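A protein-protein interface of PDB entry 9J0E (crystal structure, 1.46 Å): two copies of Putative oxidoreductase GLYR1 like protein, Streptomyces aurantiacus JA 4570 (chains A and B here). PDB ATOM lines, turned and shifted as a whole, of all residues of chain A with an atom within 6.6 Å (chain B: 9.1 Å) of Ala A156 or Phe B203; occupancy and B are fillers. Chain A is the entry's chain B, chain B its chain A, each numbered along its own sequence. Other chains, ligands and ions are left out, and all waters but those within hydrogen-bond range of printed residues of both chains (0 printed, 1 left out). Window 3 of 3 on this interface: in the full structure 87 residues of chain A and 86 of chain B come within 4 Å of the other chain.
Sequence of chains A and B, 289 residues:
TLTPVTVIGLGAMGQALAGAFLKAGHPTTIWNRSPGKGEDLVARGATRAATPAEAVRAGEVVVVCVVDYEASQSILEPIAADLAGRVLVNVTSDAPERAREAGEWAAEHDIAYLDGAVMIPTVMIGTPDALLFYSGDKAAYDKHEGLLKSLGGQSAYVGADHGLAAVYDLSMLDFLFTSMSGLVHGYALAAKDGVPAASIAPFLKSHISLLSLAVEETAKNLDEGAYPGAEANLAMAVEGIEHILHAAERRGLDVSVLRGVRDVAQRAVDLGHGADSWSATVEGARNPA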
ATOM      1  N   LEU A 131      -3.519 -12.504  -6.431  1.00  0.00           N
ATOM      2  CA  LEU A 131      -2.273 -12.365  -5.687  1.00  0.00           C
ATOM      3  C   LEU A 131      -1.618 -11.085  -6.166  1.00  0.00           C
ATOM      4  O   LEU A 131      -1.371 -10.929  -7.365  1.00  0.00           O
ATOM      5  CB  LEU A 131      -1.330 -13.551  -5.938  1.00  0.00           C
ATOM      6  CG  LEU A 131       0.128 -13.373  -5.466  1.00  0.00           C
ATOM      7  CD1 LEU A 131       0.215 -13.141  -3.958  1.00  0.00           C
ATOM      8  CD2 LEU A 131       0.977 -14.578  -5.862  1.00  0.00           C
ATOM      9  N   LEU A 132      -1.360 -10.172  -5.238  1.00  0.00           N
ATOM     10  CA  LEU A 132      -0.574  -8.977  -5.506  1.00  0.00           C
ATOM     11  C   LEU A 132       0.468  -8.828  -4.407  1.00  0.00           C
ATOM     12  O   LEU A 132       0.187  -9.117  -3.240  1.00  0.00           O
ATOM     13  CB  LEU A 132      -1.445  -7.703  -5.564  1.00  0.00           C
ATOM     14  CG  LEU A 132      -2.406  -7.539  -6.749  1.00  0.00           C
ATOM     15  CD1 LEU A 132      -3.709  -8.292  -6.534  1.00  0.00           C
ATOM     16  CD2 LEU A 132      -2.672  -6.063  -7.011  1.00  0.00           C
ATOM     17  N   PHE A 133       1.671  -8.391  -4.787  1.00  0.00           N
ATOM     18  CA  PHE A 133       2.743  -8.066  -3.854  1.00  0.00           C
ATOM     19  C   PHE A 133       2.860  -6.556  -3.689  1.00  0.00           C
ATOM     20  O   PHE A 133       2.599  -5.797  -4.623  1.00  0.00           O
ATOM     21  CB  PHE A 133       4.090  -8.552  -4.400  1.00  0.00           C
ATOM     22  CG  PHE A 133       4.222 -10.039  -4.471  1.00  0.00           C
ATOM     23  CD1 PHE A 133       4.089 -10.806  -3.329  1.00  0.00           C
ATOM     24  CD2 PHE A 133       4.510 -10.673  -5.679  1.00  0.00           C
ATOM     25  CE1 PHE A 133       4.230 -12.186  -3.376  1.00  0.00           C
ATOM     26  CE2 PHE A 133       4.661 -12.057  -5.731  1.00  0.00           C
ATOM     27  CZ  PHE A 133       4.511 -12.811  -4.580  1.00  0.00           C
ATOM     28  N   TYR A 134       3.293  -6.127  -2.497  1.00  0.00           N
ATOM     29  CA  TYR A 134       3.607  -4.728  -2.229  1.00  0.00           C
ATOM     30  C   TYR A 134       4.843  -4.636  -1.353  1.00  0.00           C
ATOM     31  O   TYR A 134       5.043  -5.469  -0.469  1.00  0.00           O
ATOM     32  CB  TYR A 134       2.476  -4.027  -1.466  1.00  0.00           C
ATOM     33  CG  TYR A 134       1.161  -4.069  -2.182  1.00  0.00           C
ATOM     34  CD1 TYR A 134       0.819  -3.080  -3.093  1.00  0.00           C
ATOM     35  CD2 TYR A 134       0.274  -5.105  -1.962  1.00  0.00           C
ATOM     36  CE1 TYR A 134      -0.392  -3.124  -3.771  1.00  0.00           C
ATOM     37  CE2 TYR A 134      -0.936  -5.161  -2.627  1.00  0.00           C
ATOM     38  CZ  TYR A 134      -1.260  -4.161  -3.530  1.00  0.00           C
ATOM     39  OH  TYR A 134      -2.467  -4.209  -4.204  1.00  0.00           O
ATOM     40  N   SER A 135       5.655  -3.611  -1.589  1.00  0.00           N
ATOM     41  CA  SER A 135       6.777  -3.301  -0.714  1.00  0.00           C
ATOM     42  C   SER A 135       6.906  -1.788  -0.626  1.00  0.00           C
ATOM     43  O   SER A 135       6.444  -1.052  -1.502  1.00  0.00           O
ATOM     44  CB  SER A 135       8.082  -3.959  -1.196  1.00  0.00           C
ATOM     45  OG  SER A 135       8.485  -3.477  -2.470  1.00  0.00           O
ATOM     46  N   TYR A 141       0.472   1.085   3.550  1.00  0.00           N
ATOM     47  CA  TYR A 141      -0.181  -0.196   3.318  1.00  0.00           C
ATOM     48  C   TYR A 141      -1.223  -0.483   4.396  1.00  0.00           C
ATOM     49  O   TYR A 141      -2.368  -0.837   4.092  1.00  0.00           O
ATOM     50  CB  TYR A 141       0.849  -1.329   3.231  1.00  0.00           C
ATOM     51  CG  TYR A 141       0.156  -2.643   2.953  1.00  0.00           C
ATOM     52  CD1 TYR A 141      -0.103  -3.049   1.647  1.00  0.00           C
ATOM     53  CD2 TYR A 141      -0.289  -3.452   3.990  1.00  0.00           C
ATOM     54  CE1 TYR A 141      -0.767  -4.229   1.388  1.00  0.00           C
ATOM     55  CE2 TYR A 141      -0.951  -4.638   3.736  1.00  0.00           C
ATOM     56  CZ  TYR A 141      -1.182  -5.020   2.434  1.00  0.00           C
ATOM     57  OH  TYR A 141      -1.846  -6.198   2.180  1.00  0.00           O
ATOM     58  N   GLY A 153      -8.042 -11.458  -2.668  1.00  0.00           N
ATOM     59  CA  GLY A 153      -7.782 -12.146  -1.421  1.00  0.00           C
ATOM     60  C   GLY A 153      -6.346 -12.099  -0.939  1.00  0.00           C
ATOM     61  O   GLY A 153      -6.103 -11.675   0.190  1.00  0.00           O
ATOM     62  N   GLN A 154      -5.389 -12.523  -1.768  1.00  0.00           N
ATOM     63  CA  GLN A 154      -3.980 -12.561  -1.368  1.00  0.00           C
ATOM     64  C   GLN A 154      -3.323 -11.223  -1.707  1.00  0.00           C
ATOM     65  O   GLN A 154      -2.908 -10.985  -2.840  1.00  0.00           O
ATOM     66  CB  GLN A 154      -3.262 -13.738  -2.021  1.00  0.00           C
ATOM     67  CG  GLN A 154      -2.793 -14.790  -1.028  1.00  0.00           C
ATOM     68  CD  GLN A 154      -1.851 -15.817  -1.641  1.00  0.00           C
ATOM     69  OE1 GLN A 154      -2.156 -16.432  -2.666  1.00  0.00           O
ATOM     70  NE2 GLN A 154      -0.696 -16.002  -1.011  1.00  0.00           N
ATOM     71  N   SER A 155      -3.231 -10.347  -0.717  1.00  0.00           N
ATOM     72  CA  SER A 155      -2.572  -9.051  -0.849  1.00  0.00           C
ATOM     73  C   SER A 155      -1.400  -9.062   0.123  1.00  0.00           C
ATOM     74  O   SER A 155      -1.593  -8.954   1.338  1.00  0.00           O
ATOM     75  CB  SER A 155      -3.565  -7.931  -0.535  1.00  0.00           C
ATOM     76  OG  SER A 155      -2.933  -6.704  -0.221  1.00  0.00           O
ATOM     77  N   ALA A 156      -0.186  -9.201  -0.405  1.00  0.00           N
ATOM     78  CA  ALA A 156       0.971  -9.592   0.394  1.00  0.00           C
ATOM     79  C   ALA A 156       1.982  -8.453   0.455  1.00  0.00           C
ATOM     80  O   ALA A 156       2.722  -8.221  -0.506  1.00  0.00           O
ATOM     81  CB  ALA A 156       1.607 -10.862  -0.176  1.00  0.00           C
ATOM     82  N   TYR A 157       2.033  -7.765   1.594  1.00  0.00           N
ATOM     83  CA  TYR A 157       3.106  -6.812   1.854  1.00  0.00           C
ATOM     84  C   TYR A 157       4.359  -7.590   2.250  1.00  0.00           C
ATOM     85  O   TYR A 157       4.341  -8.346   3.227  1.00  0.00           O
ATOM     86  CB  TYR A 157       2.692  -5.848   2.967  1.00  0.00           C
ATOM     87  CG  TYR A 157       3.805  -4.905   3.371  1.00  0.00           C
ATOM     88  CD1 TYR A 157       4.680  -5.235   4.399  1.00  0.00           C
ATOM     89  CD2 TYR A 157       3.991  -3.699   2.710  1.00  0.00           C
ATOM     90  CE1 TYR A 157       5.711  -4.384   4.761  1.00  0.00           C
ATOM     91  CE2 TYR A 157       5.017  -2.829   3.075  1.00  0.00           C
ATOM     92  CZ  TYR A 157       5.868  -3.180   4.100  1.00  0.00           C
ATOM     93  OH  TYR A 157       6.891  -2.326   4.462  1.00  0.00           O
ATOM     94  N   VAL A 158       5.446  -7.419   1.496  1.00  0.00           N
ATOM     95  CA  VAL A 158       6.623  -8.266   1.682  1.00  0.00           C
ATOM     96  C   VAL A 158       7.773  -7.620   2.461  1.00  0.00           C
ATOM     97  O   VAL A 158       8.647  -8.350   2.955  1.00  0.00           O
ATOM     98  CB  VAL A 158       7.115  -8.906   0.361  1.00  0.00           C
ATOM     99  CG1 VAL A 158       6.071  -9.891  -0.191  1.00  0.00           C
ATOM    100  CG2 VAL A 158       7.466  -7.846  -0.669  1.00  0.00           C
ATOM    101  N   GLY A 159       7.807  -6.299   2.581  1.00  0.00           N
ATOM    102  CA  GLY A 159       8.864  -5.649   3.337  1.00  0.00           C
ATOM    103  C   GLY A 159       9.058  -4.209   2.911  1.00  0.00           C
ATOM    104  O   GLY A 159       8.399  -3.706   2.001  1.00  0.00           O
ATOM    105  N   ALA A 165       9.179  -6.236  -3.752  1.00  0.00           N
ATOM    106  CA  ALA A 165       8.061  -6.783  -4.517  1.00  0.00           C
ATOM    107  C   ALA A 165       8.489  -7.128  -5.937  1.00  0.00           C
ATOM    108  O   ALA A 165       8.058  -8.149  -6.497  1.00  0.00           O
ATOM    109  CB  ALA A 165       6.896  -5.786  -4.535  1.00  0.00           C
ATOM    110  N   TYR A 168      10.229 -10.570  -6.033  1.00  0.00           N
ATOM    111  CA  TYR A 168       9.248 -11.649  -6.023  1.00  0.00           C
ATOM    112  C   TYR A 168       8.573 -11.760  -7.383  1.00  0.00           C
ATOM    113  O   TYR A 168       8.414 -12.866  -7.919  1.00  0.00           O
ATOM    114  CB  TYR A 168       8.200 -11.386  -4.936  1.00  0.00           C
ATOM    115  CG  TYR A 168       8.610 -11.770  -3.522  1.00  0.00           C
ATOM    116  CD1 TYR A 168       9.509 -10.998  -2.806  1.00  0.00           C
ATOM    117  CD2 TYR A 168       8.079 -12.896  -2.902  1.00  0.00           C
ATOM    118  CE1 TYR A 168       9.879 -11.343  -1.514  1.00  0.00           C
ATOM    119  CE2 TYR A 168       8.443 -13.247  -1.610  1.00  0.00           C
ATOM    120  CZ  TYR A 168       9.340 -12.459  -0.922  1.00  0.00           C
ATOM    121  OH  TYR A 168       9.720 -12.782   0.366  1.00  0.00           O
ATOM    122  N   MET A 172       9.008 -15.036 -10.058  1.00  0.00           N
ATOM    123  CA  MET A 172       7.869 -15.867 -10.420  1.00  0.00           C
ATOM    124  C   MET A 172       7.586 -15.801 -11.916  1.00  0.00           C
ATOM    125  O   MET A 172       7.282 -16.826 -12.542  1.00  0.00           O
ATOM    126  CB  MET A 172       6.650 -15.446  -9.605  1.00  0.00           C
ATOM    127  CG  MET A 172       6.806 -15.722  -8.116  1.00  0.00           C
ATOM    128  SD  MET A 172       5.329 -15.241  -7.199  1.00  0.00           S
ATOM    129  CE  MET A 172       4.094 -16.270  -8.006  1.00  0.00           C
ATOM    130  N   TYR B 187      14.169 -19.213  -8.983  1.00  0.00           N
ATOM    131  CA  TYR B 187      14.758 -19.274  -7.648  1.00  0.00           C
ATOM    132  C   TYR B 187      16.170 -18.700  -7.642  1.00  0.00           C
ATOM    133  O   TYR B 187      16.567 -18.025  -6.685  1.00  0.00           O
ATOM    134  CB  TYR B 187      14.772 -20.710  -7.130  1.00  0.00           C
ATOM    135  CG  TYR B 187      13.435 -21.265  -6.664  1.00  0.00           C
ATOM    136  CD1 TYR B 187      12.454 -20.442  -6.113  1.00  0.00           C
ATOM    137  CD2 TYR B 187      13.179 -22.627  -6.752  1.00  0.00           C
ATOM    138  CE1 TYR B 187      11.251 -20.973  -5.675  1.00  0.00           C
ATOM    139  CE2 TYR B 187      11.988 -23.165  -6.317  1.00  0.00           C
ATOM    140  CZ  TYR B 187      11.027 -22.334  -5.780  1.00  0.00           C
ATOM    141  OH  TYR B 187       9.847 -22.880  -5.343  1.00  0.00           O
ATOM    142  N   VAL B 195      16.652 -13.434  -1.519  1.00  0.00           N
ATOM    143  CA  VAL B 195      15.355 -14.007  -1.180  1.00  0.00           C
ATOM    144  C   VAL B 195      15.492 -15.524  -1.243  1.00  0.00           C
ATOM    145  O   VAL B 195      15.768 -16.067  -2.320  1.00  0.00           O
ATOM    146  CB  VAL B 195      14.250 -13.504  -2.121  1.00  0.00           C
ATOM    147  CG1 VAL B 195      12.919 -14.186  -1.799  1.00  0.00           C
ATOM    148  CG2 VAL B 195      14.125 -11.974  -2.001  1.00  0.00           C
ATOM    149  N   PRO B 196      15.337 -16.241  -0.131  1.00  0.00           N
ATOM    150  CA  PRO B 196      15.431 -17.700  -0.187  1.00  0.00           C
ATOM    151  C   PRO B 196      14.252 -18.279  -0.948  1.00  0.00           C
ATOM    152  O   PRO B 196      13.155 -17.710  -0.992  1.00  0.00           O
ATOM    153  CB  PRO B 196      15.399 -18.120   1.286  1.00  0.00           C
ATOM    154  CG  PRO B 196      14.657 -16.988   1.982  1.00  0.00           C
ATOM    155  CD  PRO B 196      15.022 -15.742   1.225  1.00  0.00           C
ATOM    156  N   ALA B 197      14.489 -19.436  -1.556  1.00  0.00           N
ATOM    157  CA  ALA B 197      13.427 -20.059  -2.336  1.00  0.00           C
ATOM    158  C   ALA B 197      12.218 -20.400  -1.470  1.00  0.00           C
ATOM    159  O   ALA B 197      11.081 -20.393  -1.960  1.00  0.00           O
ATOM    160  CB  ALA B 197      13.987 -21.299  -3.035  1.00  0.00           C
ATOM    161  N   ALA B 198      12.438 -20.688  -0.183  1.00  0.00           N
ATOM    162  CA  ALA B 198      11.330 -20.989   0.722  1.00  0.00           C
ATOM    163  C   ALA B 198      10.335 -19.843   0.804  1.00  0.00           C
ATOM    164  O   ALA B 198       9.155 -20.073   1.097  1.00  0.00           O
ATOM    165  CB  ALA B 198      11.857 -21.293   2.126  1.00  0.00           C
ATOM    166  N   SER B 199      10.784 -18.609   0.575  1.00  0.00           N
ATOM    167  CA  SER B 199       9.864 -17.477   0.622  1.00  0.00           C
ATOM    168  C   SER B 199       9.050 -17.337  -0.659  1.00  0.00           C
ATOM    169  O   SER B 199       7.915 -16.846  -0.615  1.00  0.00           O
ATOM    170  CB  SER B 199      10.625 -16.189   0.927  1.00  0.00           C
ATOM    171  OG  SER B 199      11.177 -16.240   2.231  1.00  0.00           O
ATOM    172  N   ILE B 200       9.604 -17.762  -1.798  1.00  0.00           N
ATOM    173  CA  ILE B 200       8.899 -17.689  -3.078  1.00  0.00           C
ATOM    174  C   ILE B 200       7.923 -18.850  -3.229  1.00  0.00           C
ATOM    175  O   ILE B 200       6.832 -18.694  -3.796  1.00  0.00           O
ATOM    176  CB  ILE B 200       9.930 -17.670  -4.226  1.00  0.00           C
ATOM    177  CG1 ILE B 200      10.887 -16.478  -4.102  1.00  0.00           C
ATOM    178  CG2 ILE B 200       9.240 -17.701  -5.599  1.00  0.00           C
ATOM    179  CD1 ILE B 200      10.226 -15.141  -4.313  1.00  0.00           C
ATOM    180  N   ALA B 201       8.294 -20.026  -2.724  1.00  0.00           N
ATOM    181  CA  ALA B 201       7.564 -21.254  -3.039  1.00  0.00           C
ATOM    182  C   ALA B 201       6.075 -21.190  -2.722  1.00  0.00           C
ATOM    183  O   ALA B 201       5.269 -21.650  -3.552  1.00  0.00           O
ATOM    184  CB  ALA B 201       8.260 -22.451  -2.380  1.00  0.00           C
ATOM    185  N   PRO B 202       5.636 -20.682  -1.567  1.00  0.00           N
ATOM    186  CA  PRO B 202       4.186 -20.662  -1.302  1.00  0.00           C
ATOM    187  C   PRO B 202       3.412 -19.873  -2.336  1.00  0.00           C
ATOM    188  O   PRO B 202       2.300 -20.264  -2.709  1.00  0.00           O
ATOM    189  CB  PRO B 202       4.089 -20.024   0.092  1.00  0.00           C
ATOM    190  CG  PRO B 202       5.446 -20.207   0.699  1.00  0.00           C
ATOM    191  CD  PRO B 202       6.411 -20.118  -0.450  1.00  0.00           C
ATOM    192  N   PHE B 203       3.979 -18.772  -2.826  1.00  0.00           N
ATOM    193  CA  PHE B 203       3.270 -17.961  -3.808  1.00  0.00           C
ATOM    194  C   PHE B 203       3.192 -18.650  -5.160  1.00  0.00           C
ATOM    195  O   PHE B 203       2.231 -18.434  -5.908  1.00  0.00           O
ATOM    196  CB  PHE B 203       3.934 -16.588  -3.926  1.00  0.00           C
ATOM    197  CG  PHE B 203       3.877 -15.791  -2.656  1.00  0.00           C
ATOM    198  CD1 PHE B 203       2.664 -15.313  -2.187  1.00  0.00           C
ATOM    199  CD2 PHE B 203       5.030 -15.526  -1.926  1.00  0.00           C
ATOM    200  CE1 PHE B 203       2.596 -14.569  -1.009  1.00  0.00           C
ATOM    201  CE2 PHE B 203       4.968 -14.792  -0.756  1.00  0.00           C
ATOM    202  CZ  PHE B 203       3.739 -14.314  -0.297  1.00  0.00           C
ATOM    203  N   LEU B 204       4.177 -19.485  -5.491  1.00  0.00           N
ATOM    204  CA  LEU B 204       4.128 -20.190  -6.767  1.00  0.00           C
ATOM    205  C   LEU B 204       2.928 -21.115  -6.883  1.00  0.00           C
ATOM    206  O   LEU B 204       2.575 -21.516  -8.001  1.00  0.00           O
ATOM    207  CB  LEU B 204       5.436 -20.937  -7.009  1.00  0.00           C
ATOM    208  CG  LEU B 204       6.598 -20.063  -7.483  1.00  0.00           C
ATOM    209  CD1 LEU B 204       7.909 -20.837  -7.443  1.00  0.00           C
ATOM    210  CD2 LEU B 204       6.303 -19.591  -8.894  1.00  0.00           C
ATOM    211  N   LYS B 205       2.269 -21.456  -5.773  1.00  0.00           N
ATOM    212  CA  LYS B 205       1.017 -22.199  -5.892  1.00  0.00           C
ATOM    213  C   LYS B 205       0.026 -21.480  -6.803  1.00  0.00           C
ATOM    214  O   LYS B 205      -0.761 -22.132  -7.500  1.00  0.00           O
ATOM    215  CB  LYS B 205       0.391 -22.425  -4.516  1.00  0.00           C
ATOM    216  CG  LYS B 205       1.192 -23.342  -3.616  1.00  0.00           C
ATOM    217  CD  LYS B 205       0.539 -23.447  -2.247  1.00  0.00           C
ATOM    218  CE  LYS B 205       0.818 -24.794  -1.599  1.00  0.00           C
ATOM    219  NZ  LYS B 205      -0.042 -24.990  -0.396  1.00  0.00           N
ATOM    220  N   SER B 206       0.056 -20.141  -6.818  1.00  0.00           N
ATOM    221  CA  SER B 206      -0.840 -19.384  -7.690  1.00  0.00           C
ATOM    222  C   SER B 206      -0.513 -19.626  -9.155  1.00  0.00           C
ATOM    223  O   SER B 206      -1.412 -19.650 -10.005  1.00  0.00           O
ATOM    224  CB  SER B 206      -0.738 -17.891  -7.385  1.00  0.00           C
ATOM    225  OG  SER B 206      -1.144 -17.606  -6.063  1.00  0.00           O
ATOM    226  N   HIS B 207       0.772 -19.785  -9.474  1.00  0.00           N
ATOM    227  CA  HIS B 207       1.150 -20.005 -10.862  1.00  0.00           C
ATOM    228  C   HIS B 207       0.946 -21.448 -11.290  1.00  0.00           C
ATOM    229  O   HIS B 207       0.689 -21.703 -12.472  1.00  0.00           O
ATOM    230  CB  HIS B 207       2.568 -19.498 -11.117  1.00  0.00           C
ATOM    231  CG  HIS B 207       2.629 -18.014 -11.240  1.00  0.00           C
ATOM    232  ND1 HIS B 207       3.790 -17.327 -11.520  1.00  0.00           N
ATOM    233  CD2 HIS B 207       1.654 -17.081 -11.124  1.00  0.00           C
ATOM    234  CE1 HIS B 207       3.529 -16.033 -11.564  1.00  0.00           C
ATOM    235  NE2 HIS B 207       2.241 -15.856 -11.323  1.00  0.00           N
ATOM    236  N   ILE B 208       1.041 -22.398 -10.356  1.00  0.00           N
ATOM    237  CA  ILE B 208       0.633 -23.769 -10.654  1.00  0.00           C
ATOM    238  C   ILE B 208      -0.843 -23.806 -11.043  1.00  0.00           C
ATOM    239  O   ILE B 208      -1.218 -24.398 -12.060  1.00  0.00           O
ATOM    240  CB  ILE B 208       0.943 -24.698  -9.467  1.00  0.00           C
ATOM    241  CG1 ILE B 208       2.458 -24.748  -9.196  1.00  0.00           C
ATOM    242  CG2 ILE B 208       0.377 -26.097  -9.723  1.00  0.00           C
ATOM    243  CD1 ILE B 208       3.279 -25.434 -10.289  1.00  0.00           C
ATOM    244  N   SER B 209      -1.702 -23.155 -10.246  1.00  0.00           N
ATOM    245  CA  SER B 209      -3.127 -23.097 -10.574  1.00  0.00           C
ATOM    246  C   SER B 209      -3.353 -22.428 -11.923  1.00  0.00           C
ATOM    247  O   SER B 209      -4.185 -22.884 -12.727  1.00  0.00           O
ATOM    248  CB  SER B 209      -3.882 -22.357  -9.469  1.00  0.00           C
ATOM    249  OG  SER B 209      -3.776 -23.057  -8.242  1.00  0.00           O
ATOM    250  N   LEU B 210      -2.607 -21.358 -12.203  1.00  0.00           N
ATOM    251  CA  LEU B 210      -2.723 -20.687 -13.489  1.00  0.00           C
ATOM    252  C   LEU B 210      -2.315 -21.611 -14.627  1.00  0.00           C
ATOM    253  O   LEU B 210      -2.977 -21.658 -15.670  1.00  0.00           O
ATOM    254  CB  LEU B 210      -1.872 -19.422 -13.484  1.00  0.00           C
ATOM    255  CG  LEU B 210      -1.876 -18.531 -14.720  1.00  0.00           C
ATOM    256  CD1 LEU B 210      -3.305 -18.196 -15.134  1.00  0.00           C
ATOM    257  CD2 LEU B 210      -1.084 -17.268 -14.407  1.00  0.00           C
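CD1 of Phe B203 touches CD1 of Leu A131, at 3.7 Å.
OG of Ser B206 touches CD2 of Leu A131, 3.7 Å away.
NE2 of Gln A154 touches CE1 of Phe B203 (3.6 Å).
Gln A154 touches Ser B206 (OE1 to OG, 3.7 Å).
Ala A156 touches Phe B203.
Tyr A168 touches Ser B199 (OH to CB, 3.6 Å).
Tyr A168 touches Ile B200 (CD2 to CD1, 3.4 Å).
Phe B203 touches Met A172.
Met A172 touches Leu B204 (CG to CD2, 3.98 Å).
Met A172 touches His B207.
No position is printed for both chains.
Of the 12 pairs that touch across the chains among the printed residues, none has its exchanged pair printed and touching as well.
Of the 16 printed residues of chain A, 6 touch a printed residue of chain B.
Printed residues of chain A that touch a printed residue of chain B: Leu A131, Phe A133, Gln A154, Ala A156, Tyr A168 and Met A172.
Hydrophobic or aromatic side chains of chain A within 4 Å of the printed part of chain B: Leu A131, Phe A133, Ala A156, Tyr A168 and Met A172.
Of the 17 printed residues of chain B, 6 touch a printed residue of chain A.
Hydrophobic or aromatic side chains of chain B within 4 Å of the printed part of chain A: Ile B200, Phe B203, Leu B204 and His B207.
Among the printed residues, 12 pairs touch across the chains.
Among the printed residues, no Asp or Glu carboxylate lies within 4 Å of a Lys or Arg side-chain nitrogen of the other chain.
The backbone NH of Ala A156 is in hydrogen-bond range of the backbone carbonyl oxygen of Leu A132 (2.9 Å).
The backbone carbonyl oxygen (O) of Phe B203 lies close to the side-chain hydroxyl (OG) of Ser B206 (3.5 Å).
The backbone NH (N) of Tyr A134 is in hydrogen-bond range of the backbone carbonyl oxygen (O) of Ala A156 (2.9 Å).
O of Gln A154 sits at hydrogen-bond distance from N of Leu A132 (3.0 Å).
Ala A156 touches one residue of chain B.
Phe B203 touches six residues of chain A.
Ser A155 touches none of the printed residues of chain B.
Printed residues of chain A within 4 Å of His B207: Met A172 (3.6 Å).
Of the printed residues of chain B, Gln A154 touches Phe B203 (3.6 Å) and Ser B206 (3.7 Å).
Ala B198 touches none of the printed residues of chain A.
Pro B196 touches none of the printed residues of chain A.
The nearest residue of chain A that does not touch Phe B203 is Val A158 (5.0 Å).
The nearest printed residue of chain B that does not touch Phe A133 is Ile B200 (6.2 Å).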
